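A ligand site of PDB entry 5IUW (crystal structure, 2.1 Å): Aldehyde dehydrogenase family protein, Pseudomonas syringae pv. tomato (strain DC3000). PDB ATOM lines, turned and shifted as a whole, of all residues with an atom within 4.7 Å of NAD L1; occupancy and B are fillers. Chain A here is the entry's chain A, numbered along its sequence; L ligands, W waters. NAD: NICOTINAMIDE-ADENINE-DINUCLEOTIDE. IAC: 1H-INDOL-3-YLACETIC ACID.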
ATOM      1  N   ILE A 164      -8.913 -14.921  15.980  1.00  0.00           N
ATOM      2  CA  ILE A 164      -9.874 -13.889  15.676  1.00  0.00           C
ATOM      3  C   ILE A 164     -11.037 -14.002  16.662  1.00  0.00           C
ATOM      4  O   ILE A 164     -11.685 -15.043  16.736  1.00  0.00           O
ATOM      5  CB  ILE A 164     -10.387 -14.021  14.222  1.00  0.00           C
ATOM      6  CG1 ILE A 164      -9.209 -13.964  13.241  1.00  0.00           C
ATOM      7  CG2 ILE A 164     -11.458 -12.981  13.946  1.00  0.00           C
ATOM      8  CD1 ILE A 164      -9.601 -14.215  11.777  1.00  0.00           C
ATOM      9  N   VAL A 165     -11.286 -12.962  17.437  1.00  0.00           N
ATOM     10  CA  VAL A 165     -12.190 -13.065  18.571  1.00  0.00           C
ATOM     11  C   VAL A 165     -13.273 -11.966  18.597  1.00  0.00           C
ATOM     12  O   VAL A 165     -13.150 -10.951  17.891  1.00  0.00           O
ATOM     13  CB  VAL A 165     -11.377 -13.035  19.886  1.00  0.00           C
ATOM     14  CG1 VAL A 165     -10.435 -14.215  19.935  1.00  0.00           C
ATOM     15  CG2 VAL A 165     -10.620 -11.755  20.002  1.00  0.00           C
ATOM     16  N   PRO A 166     -14.335 -12.173  19.397  1.00  0.00           N
ATOM     17  CA  PRO A 166     -15.473 -11.252  19.387  1.00  0.00           C
ATOM     18  C   PRO A 166     -15.410 -10.247  20.523  1.00  0.00           C
ATOM     19  O   PRO A 166     -14.421 -10.170  21.260  1.00  0.00           O
ATOM     20  CB  PRO A 166     -16.660 -12.189  19.547  1.00  0.00           C
ATOM     21  CG  PRO A 166     -16.138 -13.230  20.512  1.00  0.00           C
ATOM     22  CD  PRO A 166     -14.634 -13.327  20.278  1.00  0.00           C
ATOM     23  N   TRP A 167     -16.471  -9.486  20.665  1.00  0.00           N
ATOM     24  CA  TRP A 167     -16.504  -8.354  21.594  1.00  0.00           C
ATOM     25  C   TRP A 167     -17.213  -8.627  22.930  1.00  0.00           C
ATOM     26  O   TRP A 167     -17.157  -7.797  23.811  1.00  0.00           O
ATOM     27  CB  TRP A 167     -17.142  -7.161  20.910  1.00  0.00           C
ATOM     28  CG  TRP A 167     -18.484  -7.447  20.300  1.00  0.00           C
ATOM     29  CD1 TRP A 167     -18.742  -7.722  18.989  1.00  0.00           C
ATOM     30  CD2 TRP A 167     -19.741  -7.499  20.984  1.00  0.00           C
ATOM     31  NE1 TRP A 167     -20.081  -7.919  18.806  1.00  0.00           N
ATOM     32  CE2 TRP A 167     -20.726  -7.790  20.012  1.00  0.00           C
ATOM     33  CE3 TRP A 167     -20.140  -7.307  22.317  1.00  0.00           C
ATOM     34  CZ2 TRP A 167     -22.076  -7.900  20.331  1.00  0.00           C
ATOM     35  CZ3 TRP A 167     -21.484  -7.426  22.626  1.00  0.00           C
ATOM     36  CH2 TRP A 167     -22.443  -7.717  21.639  1.00  0.00           C
ATOM     37  N   ASN A 168     -17.898  -9.760  23.079  1.00  0.00           N
ATOM     38  CA  ASN A 168     -18.719  -9.916  24.278  1.00  0.00           C
ATOM     39  C   ASN A 168     -17.924 -10.294  25.540  1.00  0.00           C
ATOM     40  O   ASN A 168     -18.262  -9.856  26.638  1.00  0.00           O
ATOM     41  CB  ASN A 168     -19.834 -10.925  24.022  1.00  0.00           C
ATOM     42  CG  ASN A 168     -19.332 -12.325  23.726  1.00  0.00           C
ATOM     43  OD1 ASN A 168     -18.279 -12.509  23.130  1.00  0.00           O
ATOM     44  ND2 ASN A 168     -20.114 -13.308  24.129  1.00  0.00           N
ATOM     45  N   MET A 173     -12.063 -14.337  25.990  1.00  0.00           N
ATOM     46  CA  MET A 173     -12.053 -15.133  24.763  1.00  0.00           C
ATOM     47  C   MET A 173     -10.662 -15.156  24.152  1.00  0.00           C
ATOM     48  O   MET A 173     -10.253 -16.171  23.596  1.00  0.00           O
ATOM     49  CB  MET A 173     -13.065 -14.609  23.726  1.00  0.00           C
ATOM     50  CG  MET A 173     -14.541 -14.884  24.047  1.00  0.00           C
ATOM     51  SD  MET A 173     -14.855 -16.629  24.358  1.00  0.00           S
ATOM     52  CE  MET A 173     -14.898 -16.675  26.149  1.00  0.00           C
ATOM     53  N   TRP A 176      -8.637 -17.680  26.163  1.00  0.00           N
ATOM     54  CA  TRP A 176      -9.026 -19.049  25.823  1.00  0.00           C
ATOM     55  C   TRP A 176      -8.222 -19.564  24.632  1.00  0.00           C
ATOM     56  O   TRP A 176      -7.854 -20.739  24.585  1.00  0.00           O
ATOM     57  CB  TRP A 176     -10.533 -19.127  25.509  1.00  0.00           C
ATOM     58  CG  TRP A 176     -11.402 -19.194  26.706  1.00  0.00           C
ATOM     59  CD1 TRP A 176     -11.056 -18.885  27.991  1.00  0.00           C
ATOM     60  CD2 TRP A 176     -12.758 -19.627  26.754  1.00  0.00           C
ATOM     61  NE1 TRP A 176     -12.133 -19.095  28.825  1.00  0.00           N
ATOM     62  CE2 TRP A 176     -13.181 -19.546  28.084  1.00  0.00           C
ATOM     63  CE3 TRP A 176     -13.658 -20.070  25.768  1.00  0.00           C
ATOM     64  CZ2 TRP A 176     -14.477 -19.898  28.478  1.00  0.00           C
ATOM     65  CZ3 TRP A 176     -14.938 -20.419  26.169  1.00  0.00           C
ATOM     66  CH2 TRP A 176     -15.330 -20.333  27.514  1.00  0.00           C
ATOM     67  N   LYS A 191      -6.293 -11.002  16.617  1.00  0.00           N
ATOM     68  CA  LYS A 191      -7.110 -10.031  15.920  1.00  0.00           C
ATOM     69  C   LYS A 191      -8.414  -9.764  16.682  1.00  0.00           C
ATOM     70  O   LYS A 191      -9.412 -10.440  16.490  1.00  0.00           O
ATOM     71  CB  LYS A 191      -7.335 -10.545  14.505  1.00  0.00           C
ATOM     72  CG  LYS A 191      -8.449  -9.924  13.753  1.00  0.00           C
ATOM     73  CD  LYS A 191      -8.307  -8.465  13.682  1.00  0.00           C
ATOM     74  CE  LYS A 191      -9.578  -7.913  13.119  1.00  0.00           C
ATOM     75  NZ  LYS A 191     -10.757  -8.320  13.916  1.00  0.00           N
ATOM     76  N   PRO A 192      -8.383  -8.768  17.581  1.00  0.00           N
ATOM     77  CA  PRO A 192      -9.547  -8.487  18.426  1.00  0.00           C
ATOM     78  C   PRO A 192     -10.675  -7.860  17.631  1.00  0.00           C
ATOM     79  O   PRO A 192     -10.430  -7.319  16.574  1.00  0.00           O
ATOM     80  CB  PRO A 192      -9.006  -7.503  19.451  1.00  0.00           C
ATOM     81  CG  PRO A 192      -7.950  -6.783  18.701  1.00  0.00           C
ATOM     82  CD  PRO A 192      -7.308  -7.789  17.809  1.00  0.00           C
ATOM     83  N   SER A 193     -11.892  -7.920  18.161  1.00  0.00           N
ATOM     84  CA  SER A 193     -13.012  -7.265  17.521  1.00  0.00           C
ATOM     85  C   SER A 193     -12.764  -5.773  17.414  1.00  0.00           C
ATOM     86  O   SER A 193     -12.177  -5.167  18.317  1.00  0.00           O
ATOM     87  CB  SER A 193     -14.300  -7.523  18.288  1.00  0.00           C
ATOM     88  OG  SER A 193     -15.350  -6.721  17.789  1.00  0.00           O
ATOM     89  N   GLU A 194     -13.229  -5.172  16.327  1.00  0.00           N
ATOM     90  CA  GLU A 194     -13.143  -3.722  16.199  1.00  0.00           C
ATOM     91  C   GLU A 194     -14.080  -3.030  17.200  1.00  0.00           C
ATOM     92  O   GLU A 194     -13.973  -1.829  17.409  1.00  0.00           O
ATOM     93  CB  GLU A 194     -13.476  -3.285  14.758  1.00  0.00           C
ATOM     94  CG  GLU A 194     -14.918  -3.527  14.336  1.00  0.00           C
ATOM     95  CD  GLU A 194     -15.164  -4.917  13.744  1.00  0.00           C
ATOM     96  OE1 GLU A 194     -14.354  -5.853  13.946  1.00  0.00           O
ATOM     97  OE2 GLU A 194     -16.207  -5.075  13.074  1.00  0.00           O
ATOM     98  N   TYR A 223     -10.633  -3.980  11.255  1.00  0.00           N
ATOM     99  CA  TYR A 223     -11.903  -4.552  10.870  1.00  0.00           C
ATOM    100  C   TYR A 223     -11.779  -6.013  10.440  1.00  0.00           C
ATOM    101  O   TYR A 223     -10.719  -6.466   9.994  1.00  0.00           O
ATOM    102  CB  TYR A 223     -12.513  -3.705   9.751  1.00  0.00           C
ATOM    103  CG  TYR A 223     -12.950  -2.330  10.199  1.00  0.00           C
ATOM    104  CD1 TYR A 223     -14.043  -2.171  11.047  1.00  0.00           C
ATOM    105  CD2 TYR A 223     -12.280  -1.194   9.783  1.00  0.00           C
ATOM    106  CE1 TYR A 223     -14.453  -0.929  11.460  1.00  0.00           C
ATOM    107  CE2 TYR A 223     -12.681   0.070  10.193  1.00  0.00           C
ATOM    108  CZ  TYR A 223     -13.765   0.193  11.037  1.00  0.00           C
ATOM    109  OH  TYR A 223     -14.168   1.438  11.462  1.00  0.00           O
ATOM    110  N   GLY A 224     -12.873  -6.742  10.581  1.00  0.00           N
ATOM    111  CA  GLY A 224     -12.919  -8.126  10.155  1.00  0.00           C
ATOM    112  C   GLY A 224     -12.665  -8.279   8.672  1.00  0.00           C
ATOM    113  O   GLY A 224     -11.856  -9.107   8.250  1.00  0.00           O
ATOM    114  N   HIS A 225     -13.337  -7.449   7.867  1.00  0.00           N
ATOM    115  CA  HIS A 225     -13.280  -7.594   6.420  1.00  0.00           C
ATOM    116  C   HIS A 225     -11.971  -7.073   5.830  1.00  0.00           C
ATOM    117  O   HIS A 225     -11.730  -7.248   4.643  1.00  0.00           O
ATOM    118  CB  HIS A 225     -14.470  -6.878   5.757  1.00  0.00           C
ATOM    119  CG  HIS A 225     -14.496  -5.400   5.977  1.00  0.00           C
ATOM    120  ND1 HIS A 225     -15.046  -4.826   7.108  1.00  0.00           N
ATOM    121  CD2 HIS A 225     -14.048  -4.376   5.215  1.00  0.00           C
ATOM    122  CE1 HIS A 225     -14.936  -3.517   7.023  1.00  0.00           C
ATOM    123  NE2 HIS A 225     -14.330  -3.220   5.891  1.00  0.00           N
ATOM    124  N   GLY A 228      -8.793  -9.059   9.265  1.00  0.00           N
ATOM    125  CA  GLY A 228      -9.277 -10.377   9.642  1.00  0.00           C
ATOM    126  C   GLY A 228      -9.228 -11.321   8.461  1.00  0.00           C
ATOM    127  O   GLY A 228      -8.630 -12.390   8.515  1.00  0.00           O
ATOM    128  N   LYS A 229      -9.850 -10.890   7.362  1.00  0.00           N
ATOM    129  CA  LYS A 229      -9.883 -11.614   6.118  1.00  0.00           C
ATOM    130  C   LYS A 229      -8.476 -11.873   5.595  1.00  0.00           C
ATOM    131  O   LYS A 229      -8.182 -12.968   5.140  1.00  0.00           O
ATOM    132  CB  LYS A 229     -10.722 -10.823   5.102  1.00  0.00           C
ATOM    133  CG  LYS A 229     -10.781 -11.396   3.713  1.00  0.00           C
ATOM    134  CD  LYS A 229     -11.627 -10.485   2.807  1.00  0.00           C
ATOM    135  CE  LYS A 229     -11.600 -10.949   1.368  1.00  0.00           C
ATOM    136  NZ  LYS A 229     -12.545 -10.178   0.509  1.00  0.00           N
ATOM    137  N   PHE A 242     -11.273 -19.258  15.815  1.00  0.00           N
ATOM    138  CA  PHE A 242     -12.266 -18.215  15.677  1.00  0.00           C
ATOM    139  C   PHE A 242     -13.369 -18.361  16.686  1.00  0.00           C
ATOM    140  O   PHE A 242     -13.819 -19.465  16.985  1.00  0.00           O
ATOM    141  CB  PHE A 242     -12.844 -18.233  14.250  1.00  0.00           C
ATOM    142  CG  PHE A 242     -14.018 -17.315  14.037  1.00  0.00           C
ATOM    143  CD1 PHE A 242     -15.327 -17.786  14.166  1.00  0.00           C
ATOM    144  CD2 PHE A 242     -13.811 -16.000  13.638  1.00  0.00           C
ATOM    145  CE1 PHE A 242     -16.408 -16.934  13.933  1.00  0.00           C
ATOM    146  CE2 PHE A 242     -14.893 -15.148  13.404  1.00  0.00           C
ATOM    147  CZ  PHE A 242     -16.179 -15.614  13.553  1.00  0.00           C
ATOM    148  N   THR A 243     -13.793 -17.230  17.216  1.00  0.00           N
ATOM    149  CA  THR A 243     -14.985 -17.176  18.013  1.00  0.00           C
ATOM    150  C   THR A 243     -15.807 -15.977  17.549  1.00  0.00           C
ATOM    151  O   THR A 243     -15.296 -14.855  17.478  1.00  0.00           O
ATOM    152  CB  THR A 243     -14.672 -17.080  19.500  1.00  0.00           C
ATOM    153  OG1 THR A 243     -13.968 -18.263  19.919  1.00  0.00           O
ATOM    154  CG2 THR A 243     -15.940 -16.982  20.264  1.00  0.00           C
ATOM    155  N   GLY A 244     -17.063 -16.232  17.190  1.00  0.00           N
ATOM    156  CA  GLY A 244     -17.900 -15.219  16.579  1.00  0.00           C
ATOM    157  C   GLY A 244     -19.169 -15.785  15.976  1.00  0.00           C
ATOM    158  O   GLY A 244     -19.639 -16.859  16.379  1.00  0.00           O
ATOM    159  N   SER A 245     -19.723 -15.071  15.014  1.00  0.00           N
ATOM    160  CA  SER A 245     -20.968 -15.467  14.373  1.00  0.00           C
ATOM    161  C   SER A 245     -20.823 -16.669  13.438  1.00  0.00           C
ATOM    162  O   SER A 245     -19.764 -16.919  12.871  1.00  0.00           O
ATOM    163  CB  SER A 245     -21.564 -14.285  13.601  1.00  0.00           C
ATOM    164  OG  SER A 245     -20.767 -13.973  12.480  1.00  0.00           O
ATOM    165  N   ILE A 248     -19.819 -15.701   9.791  1.00  0.00           N
ATOM    166  CA  ILE A 248     -18.408 -15.443   9.536  1.00  0.00           C
ATOM    167  C   ILE A 248     -17.601 -16.736   9.672  1.00  0.00           C
ATOM    168  O   ILE A 248     -16.630 -16.954   8.932  1.00  0.00           O
ATOM    169  CB  ILE A 248     -17.837 -14.346  10.492  1.00  0.00           C
ATOM    170  CG1 ILE A 248     -18.611 -13.038  10.333  1.00  0.00           C
ATOM    171  CG2 ILE A 248     -16.349 -14.099  10.253  1.00  0.00           C
ATOM    172  CD1 ILE A 248     -18.511 -12.426   8.944  1.00  0.00           C
ATOM    173  N   LEU A 252     -14.843 -18.244   6.941  1.00  0.00           N
ATOM    174  CA  LEU A 252     -13.482 -18.674   7.240  1.00  0.00           C
ATOM    175  C   LEU A 252     -13.132 -20.019   6.602  1.00  0.00           C
ATOM    176  O   LEU A 252     -12.000 -20.211   6.163  1.00  0.00           O
ATOM    177  CB  LEU A 252     -13.259 -18.756   8.753  1.00  0.00           C
ATOM    178  CG  LEU A 252     -13.265 -17.482   9.608  1.00  0.00           C
ATOM    179  CD1 LEU A 252     -12.416 -17.719  10.823  1.00  0.00           C
ATOM    180  CD2 LEU A 252     -12.742 -16.284   8.855  1.00  0.00           C
ATOM    181  N   TYR A 255     -12.432 -19.148   3.028  1.00  0.00           N
ATOM    182  CA  TYR A 255     -11.091 -18.552   2.934  1.00  0.00           C
ATOM    183  C   TYR A 255      -9.967 -19.574   3.000  1.00  0.00           C
ATOM    184  O   TYR A 255      -8.973 -19.450   2.301  1.00  0.00           O
ATOM    185  CB  TYR A 255     -10.870 -17.547   4.063  1.00  0.00           C
ATOM    186  CG  TYR A 255     -11.728 -16.315   3.978  1.00  0.00           C
ATOM    187  CD1 TYR A 255     -12.169 -15.823   2.753  1.00  0.00           C
ATOM    188  CD2 TYR A 255     -12.088 -15.630   5.141  1.00  0.00           C
ATOM    189  CE1 TYR A 255     -12.953 -14.679   2.696  1.00  0.00           C
ATOM    190  CE2 TYR A 255     -12.868 -14.491   5.091  1.00  0.00           C
ATOM    191  CZ  TYR A 255     -13.298 -14.024   3.882  1.00  0.00           C
ATOM    192  OH  TYR A 255     -14.070 -12.897   3.847  1.00  0.00           O
ATOM    193  N   GLU A 267     -15.740 -21.510  16.967  1.00  0.00           N
ATOM    194  CA  GLU A 267     -16.727 -21.431  18.040  1.00  0.00           C
ATOM    195  C   GLU A 267     -17.767 -20.402  17.599  1.00  0.00           C
ATOM    196  O   GLU A 267     -17.460 -19.217  17.514  1.00  0.00           O
ATOM    197  CB  GLU A 267     -16.091 -21.027  19.369  1.00  0.00           C
ATOM    198  CG  GLU A 267     -14.910 -21.890  19.814  1.00  0.00           C
ATOM    199  CD  GLU A 267     -15.304 -22.922  20.871  1.00  0.00           C
ATOM    200  OE1 GLU A 267     -16.331 -22.713  21.554  1.00  0.00           O
ATOM    201  OE2 GLU A 267     -14.585 -23.927  21.016  1.00  0.00           O
ATOM    202  N   ALA A 268     -18.985 -20.851  17.305  1.00  0.00           N
ATOM    203  CA  ALA A 268     -19.958 -19.952  16.699  1.00  0.00           C
ATOM    204  C   ALA A 268     -21.183 -19.754  17.598  1.00  0.00           C
ATOM    205  O   ALA A 268     -21.099 -19.903  18.807  1.00  0.00           O
ATOM    206  CB  ALA A 268     -20.366 -20.466  15.306  1.00  0.00           C
ATOM    207  N   GLY A 269     -22.306 -19.404  16.989  1.00  0.00           N
ATOM    208  CA  GLY A 269     -23.492 -19.012  17.737  1.00  0.00           C
ATOM    209  C   GLY A 269     -24.214 -20.117  18.484  1.00  0.00           C
ATOM    210  O   GLY A 269     -23.790 -21.273  18.476  1.00  0.00           O
ATOM    211  N   GLY A 270     -25.317 -19.756  19.134  1.00  0.00           N
ATOM    212  CA  GLY A 270     -26.120 -20.728  19.862  1.00  0.00           C
ATOM    213  C   GLY A 270     -27.548 -20.289  20.148  1.00  0.00           C
ATOM    214  O   GLY A 270     -27.883 -19.100  20.131  1.00  0.00           O
ATOM    215  N   CYS A 302     -22.950 -16.364  24.264  1.00  0.00           N
ATOM    216  CA  CYS A 302     -23.213 -17.381  23.262  1.00  0.00           C
ATOM    217  C   CYS A 302     -24.048 -18.539  23.812  1.00  0.00           C
ATOM    218  O   CYS A 302     -24.842 -19.134  23.092  1.00  0.00           O
ATOM    219  CB  CYS A 302     -21.895 -17.914  22.704  1.00  0.00           C
ATOM    220  SG  CYS A 302     -20.855 -18.796  23.909  1.00  0.00           S
ATOM    221  N   GLU A 401     -30.661 -16.675  16.871  1.00  0.00           N
ATOM    222  CA  GLU A 401     -29.886 -16.082  17.960  1.00  0.00           C
ATOM    223  C   GLU A 401     -30.098 -14.568  17.996  1.00  0.00           C
ATOM    224  O   GLU A 401     -29.927 -13.889  16.992  1.00  0.00           O
ATOM    225  CB  GLU A 401     -28.402 -16.390  17.811  1.00  0.00           C
ATOM    226  CG  GLU A 401     -27.586 -15.911  19.011  1.00  0.00           C
ATOM    227  CD  GLU A 401     -26.114 -16.285  18.943  1.00  0.00           C
ATOM    228  OE1 GLU A 401     -25.542 -16.312  17.830  1.00  0.00           O
ATOM    229  OE2 GLU A 401     -25.528 -16.572  20.021  1.00  0.00           O
ATOM    230  N   PHE A 403     -28.912 -12.440  20.788  1.00  0.00           N
ATOM    231  CA  PHE A 403     -27.751 -11.833  21.444  1.00  0.00           C
ATOM    232  C   PHE A 403     -28.191 -10.543  22.146  1.00  0.00           C
ATOM    233  O   PHE A 403     -27.546  -9.510  22.068  1.00  0.00           O
ATOM    234  CB  PHE A 403     -26.615 -11.576  20.432  1.00  0.00           C
ATOM    235  CG  PHE A 403     -25.255 -11.950  20.969  1.00  0.00           C
ATOM    236  CD1 PHE A 403     -24.978 -13.244  21.369  1.00  0.00           C
ATOM    237  CD2 PHE A 403     -24.232 -10.999  21.067  1.00  0.00           C
ATOM    238  CE1 PHE A 403     -23.738 -13.599  21.878  1.00  0.00           C
ATOM    239  CE2 PHE A 403     -22.979 -11.349  21.560  1.00  0.00           C
ATOM    240  CZ  PHE A 403     -22.730 -12.652  21.969  1.00  0.00           C
ATOM    241  N   LEU A 429     -24.543 -25.544  21.066  1.00  0.00           N
ATOM    242  CA  LEU A 429     -23.438 -25.084  21.905  1.00  0.00           C
ATOM    243  C   LEU A 429     -23.602 -25.572  23.344  1.00  0.00           C
ATOM    244  O   LEU A 429     -22.674 -26.085  23.953  1.00  0.00           O
ATOM    245  CB  LEU A 429     -23.347 -23.556  21.847  1.00  0.00           C
ATOM    246  CG  LEU A 429     -22.082 -22.926  22.404  1.00  0.00           C
ATOM    247  CD1 LEU A 429     -20.867 -23.490  21.687  1.00  0.00           C
ATOM    248  CD2 LEU A 429     -22.173 -21.440  22.211  1.00  0.00           C
ATOM    249  N   PHE A 467     -15.234 -26.888  25.937  1.00  0.00           N
ATOM    250  CA  PHE A 467     -16.347 -26.019  25.609  1.00  0.00           C
ATOM    251  C   PHE A 467     -16.349 -25.784  24.101  1.00  0.00           C
ATOM    252  O   PHE A 467     -15.325 -25.461  23.536  1.00  0.00           O
ATOM    253  CB  PHE A 467     -16.211 -24.690  26.371  1.00  0.00           C
ATOM    254  CG  PHE A 467     -17.310 -23.708  26.108  1.00  0.00           C
ATOM    255  CD1 PHE A 467     -17.294 -22.915  24.974  1.00  0.00           C
ATOM    256  CD2 PHE A 467     -18.335 -23.543  27.033  1.00  0.00           C
ATOM    257  CE1 PHE A 467     -18.302 -22.007  24.727  1.00  0.00           C
ATOM    258  CE2 PHE A 467     -19.351 -22.613  26.794  1.00  0.00           C
ATOM    259  CZ  PHE A 467     -19.322 -21.851  25.643  1.00  0.00           C
HETATM  260  PA  NAD L   1     -18.643 -11.544  14.255  1.00  0.00           P
HETATM  261  O1A NAD L   1     -18.622 -12.859  13.525  1.00  0.00           O
HETATM  262  O2A NAD L   1     -19.342 -10.509  13.443  1.00  0.00           O
HETATM  263  O5B NAD L   1     -17.133 -11.064  14.474  1.00  0.00           O
HETATM  264  C5B NAD L   1     -16.267 -11.872  15.296  1.00  0.00           C
HETATM  265  C4B NAD L   1     -14.796 -11.666  14.785  1.00  0.00           C
HETATM  266  O4B NAD L   1     -14.703 -12.014  13.523  1.00  0.00           O
HETATM  267  C3B NAD L   1     -14.451 -10.196  14.869  1.00  0.00           C
HETATM  268  O3B NAD L   1     -13.178 -10.057  15.337  1.00  0.00           O
HETATM  269  C2B NAD L   1     -14.600  -9.748  13.387  1.00  0.00           C
HETATM  270  O2B NAD L   1     -13.874  -8.457  13.168  1.00  0.00           O
HETATM  271  C1B NAD L   1     -14.130 -10.754  12.718  1.00  0.00           C
HETATM  272  N9A NAD L   1     -14.589 -10.767  11.337  1.00  0.00           N
HETATM  273  C8A NAD L   1     -15.725 -10.217  10.847  1.00  0.00           C
HETATM  274  N7A NAD L   1     -15.752 -10.437   9.516  1.00  0.00           N
HETATM  275  C5A NAD L   1     -14.628 -11.120   9.162  1.00  0.00           C
HETATM  276  C6A NAD L   1     -14.156 -11.600   7.955  1.00  0.00           C
HETATM  277  N6A NAD L   1     -14.765 -11.477   6.695  1.00  0.00           N
HETATM  278  N1A NAD L   1     -12.992 -12.260   7.872  1.00  0.00           N
HETATM  279  C2A NAD L   1     -12.284 -12.461   9.001  1.00  0.00           C
HETATM  280  N3A NAD L   1     -12.730 -11.992  10.213  1.00  0.00           N
HETATM  281  C4A NAD L   1     -13.899 -11.326  10.289  1.00  0.00           C
HETATM  282  O3  NAD L   1     -19.352 -11.778  15.649  1.00  0.00           O
HETATM  283  PN  NAD L   1     -19.595 -10.665  16.794  1.00  0.00           P
HETATM  284  O1N NAD L   1     -20.144  -9.413  16.145  1.00  0.00           O
HETATM  285  O2N NAD L   1     -18.253 -10.354  17.424  1.00  0.00           O
HETATM  286  O5D NAD L   1     -20.708 -11.169  17.826  1.00  0.00           O
HETATM  287  C5D NAD L   1     -20.515 -12.252  18.740  1.00  0.00           C
HETATM  288  C4D NAD L   1     -20.898 -13.649  18.111  1.00  0.00           C
HETATM  289  O4D NAD L   1     -19.993 -14.470  18.539  1.00  0.00           O
HETATM  290  C3D NAD L   1     -22.219 -14.239  18.600  1.00  0.00           C
HETATM  291  O3D NAD L   1     -22.877 -14.917  17.614  1.00  0.00           O
HETATM  292  C2D NAD L   1     -21.788 -15.236  19.708  1.00  0.00           C
HETATM  293  O2D NAD L   1     -22.789 -16.355  19.910  1.00  0.00           O
HETATM  294  C1D NAD L   1     -20.695 -15.711  19.281  1.00  0.00           C
HETATM  295  N1N NAD L   1     -19.885 -16.172  20.387  1.00  0.00           N
HETATM  296  C2N NAD L   1     -19.522 -17.505  20.472  1.00  0.00           C
HETATM  297  C3N NAD L   1     -18.753 -17.947  21.547  1.00  0.00           C
HETATM  298  C7N NAD L   1     -18.351 -19.419  21.641  1.00  0.00           C
HETATM  299  O7N NAD L   1     -18.926 -20.241  20.940  1.00  0.00           O
HETATM  300  N7N NAD L   1     -17.362 -19.830  22.517  1.00  0.00           N
HETATM  301  C4N NAD L   1     -18.351 -17.050  22.530  1.00  0.00           C
HETATM  302  C5N NAD L   1     -18.710 -15.722  22.452  1.00  0.00           C
HETATM  303  C6N NAD L   1     -19.483 -15.275  21.370  1.00  0.00           C
HETATM  304  C   IAC L   2     -19.033 -18.616  30.507  1.00  0.00           C
HETATM  305  C1  IAC L   2     -18.622 -17.529  29.802  1.00  0.00           C
HETATM  306  C2  IAC L   2     -18.154 -16.368  30.478  1.00  0.00           C
HETATM  307  C3  IAC L   2     -18.138 -16.348  31.870  1.00  0.00           C
HETATM  308  C4  IAC L   2     -18.556 -17.463  32.585  1.00  0.00           C
HETATM  309  C5  IAC L   2     -19.006 -18.599  31.919  1.00  0.00           C
HETATM  310  C7  IAC L   2     -18.755 -17.807  28.446  1.00  0.00           C
HETATM  311  C8  IAC L   2     -19.256 -19.079  28.313  1.00  0.00           C
HETATM  312  C17 IAC L   2     -18.386 -16.850  27.345  1.00  0.00           C
HETATM  313  C18 IAC L   2     -19.026 -17.285  26.051  1.00  0.00           C
HETATM  314  N   IAC L   2     -19.431 -19.591  29.573  1.00  0.00           N
HETATM  315  O2  IAC L   2     -20.028 -16.666  25.593  1.00  0.00           O
HETATM  316  O3  IAC L   2     -18.503 -18.241  25.432  1.00  0.00           O
HETATM  317  O   HOH W   1     -17.432 -10.543   5.290  1.00  0.00           O
HETATM  318  O   HOH W   2     -16.990  -7.920  15.957  1.00  0.00           O
HETATM  319  O   HOH W   3     -17.610  -9.055   7.933  1.00  0.00           O
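O1A of NAD L1 lies within hydrogen-bond range of N of Ser 245 (2.9 Å). The side-chain hydroxyl of Ser 245 is in hydrogen-bond range of an oxygen (O1A) of NAD L1. The backbone carbonyl oxygen of Val 165 lies within hydrogen-bond range of an oxygen (O3B) of NAD L1, at 2.7 Å. OE2 of Glu 401 lies within hydrogen-bond range of O2D of NAD L1 (2.7 Å). The side-chain carboxylate (OE1) of Glu 194 is in hydrogen-bond range of an oxygen (O2B) of NAD L1 (2.8 Å). The indole nitrogen (NE1) of Trp 167 sits at hydrogen-bond distance from an oxygen (O1N) of NAD L1 (3.1 Å). An oxygen (O2B) of NAD L1 sits close to the backbone NH (N) of Gly 224 (3.3 Å). NZ of Lys 191 is in hydrogen-bond range of O2B of NAD L1 (3.2 Å). The side-chain carboxylate (OE1) of Glu 267 sits at hydrogen-bond distance from a nitrogen (N7N) of NAD L1 (3.2 Å). N6A of NAD L1 sits at hydrogen-bond distance from OH of Tyr 255 (3.3 Å). A nitrogen (N1A) of NAD L1 lies close to the backbone NH of Lys 229 (3.5 Å). O2 of IAC L2 lies within hydrogen-bond range of N of Cys 302 (3.2 Å). The side-chain sulfur of Cys 302 lies within hydrogen-bond range of an oxygen (O2) of IAC L2 (2.8 Å).
An oxygen (O4D) of NAD L1 sits close to the backbone carbonyl oxygen (O) of Gly 244 (3.2 Å). O of Ala 268 lies close to O7N of NAD L1. Ile 164 touches NAD L1. Pro 166 touches NAD L1 (CB to O2N, 3.2 Å). Asn 168 touches NAD L1. Met 173 touches NAD L1. CA of Ser 193 touches O3B of NAD L1, at 3.5 Å. Gly 228 touches NAD L1 (C to C2A, 3.3 Å). Phe 242 touches NAD L1. Thr 243 touches NAD L1 (CG2 to C3N, 3.2 Å). Ile 248 touches NAD L1. CD2 of Leu 252 touches C2A of NAD L1 (3.9 Å). Gly 269 touches NAD L1 (CA to O2D, 3.5 Å). Cys 302 touches NAD L1 (SG to C3N, 3.3 Å). Phe 403 touches NAD L1. Leu 429 touches NAD L1 (CD2 to O7N, 3.7 Å). CE1 of Phe 467 touches N7N of NAD L1, at 3.2 Å. Hydrophobic or aromatic side chains that line NAD L1: Ile 164, Pro 166, Trp 167, Met 173, Phe 242, Ile 248, Leu 252, Tyr 255, Phe 403, Leu 429 and Phe 467. Of the 32 residues printed, 27 come within 4 Å of NAD L1.
OG of Ser 245 lies close to N of Ile 248, at 3.3 Å. The backbone carbonyl oxygen of Lys 191 is in hydrogen-bond range of the backbone NH of Val 165, 3.3 Å away. The backbone NH (N) of Ser 193 lies within hydrogen-bond range of the backbone carbonyl oxygen (O) of Val 165, 3.3 Å away. The side-chain carboxylate (OE2) of Glu 401 is in hydrogen-bond range of the backbone NH (N) of Gly 270. O of Glu 267 lies within hydrogen-bond range of N of Gly 244 (3.0 Å). N of Glu 267 lies within hydrogen-bond range of O of Phe 242, at 2.8 Å. The backbone carbonyl oxygen of Gly 224 sits at hydrogen-bond distance from the backbone NH of Lys 229, at 2.8 Å. The backbone carbonyl oxygen (O) of Tyr 223 is in hydrogen-bond range of the backbone NH (N) of Gly 228, at 3.3 Å.
Water W2 bridges OG of Ser 193 (2.7 Å) and O2N of NAD L1 (3.1 Å).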
